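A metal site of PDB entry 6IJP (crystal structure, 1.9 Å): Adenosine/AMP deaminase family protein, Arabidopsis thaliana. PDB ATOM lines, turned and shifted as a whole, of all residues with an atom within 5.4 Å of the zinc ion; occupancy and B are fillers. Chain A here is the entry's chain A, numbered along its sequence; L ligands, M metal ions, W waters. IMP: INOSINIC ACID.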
ATOM      1  N   HIS A  34     -28.942  22.808 -16.658  1.00  0.00           N
ATOM      2  CA  HIS A  34     -28.198  22.035 -17.661  1.00  0.00           C
ATOM      3  C   HIS A  34     -27.300  22.994 -18.450  1.00  0.00           C
ATOM      4  O   HIS A  34     -27.666  23.549 -19.495  1.00  0.00           O
ATOM      5  CB  HIS A  34     -29.169  21.245 -18.534  1.00  0.00           C
ATOM      6  CG  HIS A  34     -28.523  20.272 -19.493  1.00  0.00           C
ATOM      7  ND1 HIS A  34     -29.077  19.040 -19.769  1.00  0.00           N
ATOM      8  CD2 HIS A  34     -27.417  20.372 -20.286  1.00  0.00           C
ATOM      9  CE1 HIS A  34     -28.335  18.407 -20.679  1.00  0.00           C
ATOM     10  NE2 HIS A  34     -27.335  19.200 -21.019  1.00  0.00           N
ATOM     11  N   HIS A  36     -23.104  23.062 -19.490  1.00  0.00           N
ATOM     12  CA  HIS A  36     -21.747  22.514 -19.448  1.00  0.00           C
ATOM     13  C   HIS A  36     -20.720  23.632 -19.365  1.00  0.00           C
ATOM     14  O   HIS A  36     -20.791  24.620 -20.127  1.00  0.00           O
ATOM     15  CB  HIS A  36     -21.462  21.656 -20.709  1.00  0.00           C
ATOM     16  CG  HIS A  36     -22.443  20.564 -20.977  1.00  0.00           C
ATOM     17  ND1 HIS A  36     -22.260  19.264 -20.556  1.00  0.00           N
ATOM     18  CD2 HIS A  36     -23.606  20.554 -21.706  1.00  0.00           C
ATOM     19  CE1 HIS A  36     -23.271  18.504 -20.988  1.00  0.00           C
ATOM     20  NE2 HIS A  36     -24.094  19.273 -21.673  1.00  0.00           N
ATOM     21  N   ARG A 117     -22.391  21.687 -14.768  1.00  0.00           N
ATOM     22  CA  ARG A 117     -21.831  20.355 -14.939  1.00  0.00           C
ATOM     23  C   ARG A 117     -20.525  20.434 -15.720  1.00  0.00           C
ATOM     24  O   ARG A 117     -20.361  21.302 -16.596  1.00  0.00           O
ATOM     25  CB  ARG A 117     -22.797  19.398 -15.649  1.00  0.00           C
ATOM     26  CG  ARG A 117     -23.212  19.797 -17.035  1.00  0.00           C
ATOM     27  CD  ARG A 117     -24.350  18.805 -17.569  1.00  0.00           C
ATOM     28  NE  ARG A 117     -25.634  19.064 -16.887  1.00  0.00           N
ATOM     29  CZ  ARG A 117     -26.711  18.310 -17.030  1.00  0.00           C
ATOM     30  NH1 ARG A 117     -26.653  17.191 -17.795  1.00  0.00           N
ATOM     31  NH2 ARG A 117     -27.861  18.673 -16.436  1.00  0.00           N
ATOM     32  N   SER A 210     -22.926  12.283 -20.256  1.00  0.00           N
ATOM     33  CA  SER A 210     -23.008  13.115 -21.451  1.00  0.00           C
ATOM     34  C   SER A 210     -21.847  12.722 -22.374  1.00  0.00           C
ATOM     35  O   SER A 210     -21.233  11.666 -22.209  1.00  0.00           O
ATOM     36  CB  SER A 210     -23.033  14.618 -21.078  1.00  0.00           C
ATOM     37  OG  SER A 210     -21.831  15.069 -20.454  1.00  0.00           O
ATOM     38  N   HIS A 238     -28.171  12.563 -20.151  1.00  0.00           N
ATOM     39  CA  HIS A 238     -28.479  12.873 -21.535  1.00  0.00           C
ATOM     40  C   HIS A 238     -29.174  11.666 -22.170  1.00  0.00           C
ATOM     41  O   HIS A 238     -28.588  10.580 -22.211  1.00  0.00           O
ATOM     42  CB  HIS A 238     -27.198  13.216 -22.320  1.00  0.00           C
ATOM     43  CG  HIS A 238     -26.724  14.619 -22.081  1.00  0.00           C
ATOM     44  ND1 HIS A 238     -26.252  15.047 -20.847  1.00  0.00           N
ATOM     45  CD2 HIS A 238     -26.631  15.691 -22.920  1.00  0.00           C
ATOM     46  CE1 HIS A 238     -25.893  16.323 -20.933  1.00  0.00           C
ATOM     47  NE2 HIS A 238     -26.067  16.725 -22.181  1.00  0.00           N
ATOM     48  N   GLU A 241     -30.742  11.692 -27.339  1.00  0.00           N
ATOM     49  CA  GLU A 241     -30.209  12.731 -28.235  1.00  0.00           C
ATOM     50  C   GLU A 241     -30.138  12.251 -29.685  1.00  0.00           C
ATOM     51  O   GLU A 241     -30.136  13.085 -30.599  1.00  0.00           O
ATOM     52  CB  GLU A 241     -28.809  13.166 -27.816  1.00  0.00           C
ATOM     53  CG  GLU A 241     -28.701  13.842 -26.468  1.00  0.00           C
ATOM     54  CD  GLU A 241     -27.249  14.328 -26.266  1.00  0.00           C
ATOM     55  OE1 GLU A 241     -26.987  15.529 -26.500  1.00  0.00           O
ATOM     56  OE2 GLU A 241     -26.386  13.504 -25.924  1.00  0.00           O
ATOM     57  N   HIS A 261     -33.008  16.454 -22.630  1.00  0.00           N
ATOM     58  CA  HIS A 261     -33.411  16.471 -24.057  1.00  0.00           C
ATOM     59  C   HIS A 261     -34.556  15.606 -24.516  1.00  0.00           C
ATOM     60  O   HIS A 261     -35.618  16.181 -24.873  1.00  0.00           O
ATOM     61  CB  HIS A 261     -32.193  16.186 -24.911  1.00  0.00           C
ATOM     62  CG  HIS A 261     -31.164  17.197 -24.662  1.00  0.00           C
ATOM     63  ND1 HIS A 261     -31.541  18.479 -24.347  1.00  0.00           N
ATOM     64  CD2 HIS A 261     -29.818  17.132 -24.527  1.00  0.00           C
ATOM     65  CE1 HIS A 261     -30.464  19.178 -24.076  1.00  0.00           C
ATOM     66  NE2 HIS A 261     -29.404  18.391 -24.179  1.00  0.00           N
ATOM     67  N   ASP A 316     -27.786  24.572 -22.122  1.00  0.00           N
ATOM     68  CA  ASP A 316     -26.931  23.486 -22.598  1.00  0.00           C
ATOM     69  C   ASP A 316     -25.482  23.976 -22.756  1.00  0.00           C
ATOM     70  O   ASP A 316     -24.598  23.587 -21.995  1.00  0.00           O
ATOM     71  CB  ASP A 316     -27.467  22.871 -23.913  1.00  0.00           C
ATOM     72  CG  ASP A 316     -26.949  21.466 -24.154  1.00  0.00           C
ATOM     73  OD1 ASP A 316     -26.253  20.916 -23.256  1.00  0.00           O
ATOM     74  OD2 ASP A 316     -27.211  20.896 -25.253  1.00  0.00           O
ATOM     75  N   ASP A 317     -25.228  24.826 -23.764  1.00  0.00           N
ATOM     76  CA  ASP A 317     -23.888  25.336 -24.064  1.00  0.00           C
ATOM     77  C   ASP A 317     -24.082  26.766 -24.567  1.00  0.00           C
ATOM     78  O   ASP A 317     -24.126  26.998 -25.766  1.00  0.00           O
ATOM     79  CB  ASP A 317     -23.154  24.508 -25.132  1.00  0.00           C
ATOM     80  CG  ASP A 317     -22.994  23.067 -24.736  1.00  0.00           C
ATOM     81  OD1 ASP A 317     -22.085  22.789 -23.951  1.00  0.00           O
ATOM     82  OD2 ASP A 317     -23.757  22.192 -25.239  1.00  0.00           O
HETATM   83  P   IMP L   1     -17.046  20.063 -20.117  1.00  0.00           P
HETATM   84  O1P IMP L   1     -17.588  18.816 -19.473  1.00  0.00           O
HETATM   85  O2P IMP L   1     -16.965  21.166 -19.097  1.00  0.00           O
HETATM   86  O3P IMP L   1     -15.742  19.641 -20.781  1.00  0.00           O
HETATM   87  O5' IMP L   1     -18.079  20.624 -21.201  1.00  0.00           O
HETATM   88  C5' IMP L   1     -18.042  20.101 -22.526  1.00  0.00           C
HETATM   89  C4' IMP L   1     -18.538  18.680 -22.575  1.00  0.00           C
HETATM   90  O4' IMP L   1     -19.970  18.647 -22.308  1.00  0.00           O
HETATM   91  C3' IMP L   1     -18.393  18.013 -23.944  1.00  0.00           C
HETATM   92  O3' IMP L   1     -17.085  17.454 -24.127  1.00  0.00           O
HETATM   93  C2' IMP L   1     -19.522  16.974 -23.973  1.00  0.00           C
HETATM   94  O2' IMP L   1     -19.100  15.728 -23.452  1.00  0.00           O
HETATM   95  C1' IMP L   1     -20.581  17.609 -23.045  1.00  0.00           C
HETATM   96  N9  IMP L   1     -21.641  18.198 -23.858  1.00  0.00           N
HETATM   97  C8  IMP L   1     -21.824  19.521 -24.175  1.00  0.00           C
HETATM   98  N7  IMP L   1     -22.912  19.581 -24.992  1.00  0.00           N
HETATM   99  C5  IMP L   1     -23.386  18.321 -25.199  1.00  0.00           C
HETATM  100  C6  IMP L   1     -24.455  17.806 -25.956  1.00  0.00           C
HETATM  101  O6  IMP L   1     -25.048  18.509 -26.806  1.00  0.00           O
HETATM  102  N1  IMP L   1     -24.655  16.436 -25.928  1.00  0.00           N
HETATM  103  C2  IMP L   1     -23.868  15.583 -25.198  1.00  0.00           C
HETATM  104  N3  IMP L   1     -22.802  16.103 -24.484  1.00  0.00           N
HETATM  105  C4  IMP L   1     -22.584  17.446 -24.486  1.00  0.00           C
HETATM  106 ZN    ZN M   1     -25.947  18.844 -22.674  1.00  0.00          ZN
HETATM  107  O   HOH W   1     -26.843  18.420 -24.602  1.00  0.00           O
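The side-chain carboxylate of Asp 317 is in hydrogen-bond range of a nitrogen (N7) of the ligand (2.8 Å).
The side-chain carboxylate (OE1) of Glu 241 lies within hydrogen-bond range of a nitrogen (N1) of the ligand (2.6 Å).
An oxygen (O4') of the ligand sits at hydrogen-bond distance from a ring nitrogen (ND1) of His 36, at 2.9 Å.
The zinc ion is bound by NE2 of His 36 (2.1 Å), water W1 (2.2 Å), OD1 of Asp 316 (2.2 Å), NE2 of His 238 (2.2 Å) and NE2 of His 34 (2.2 Å).
The zinc ion has five donor atoms within binding distance.
His 261 touches the zinc ion.
Five residues have an atom within 4 Å of the zinc ion: His 34, His 36, His 238, His 261 and Asp 316.
A ring nitrogen (NE2) of His 261 is in hydrogen-bond range of the side-chain carboxylate (OD2) of Asp 316 (3.5 Å).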
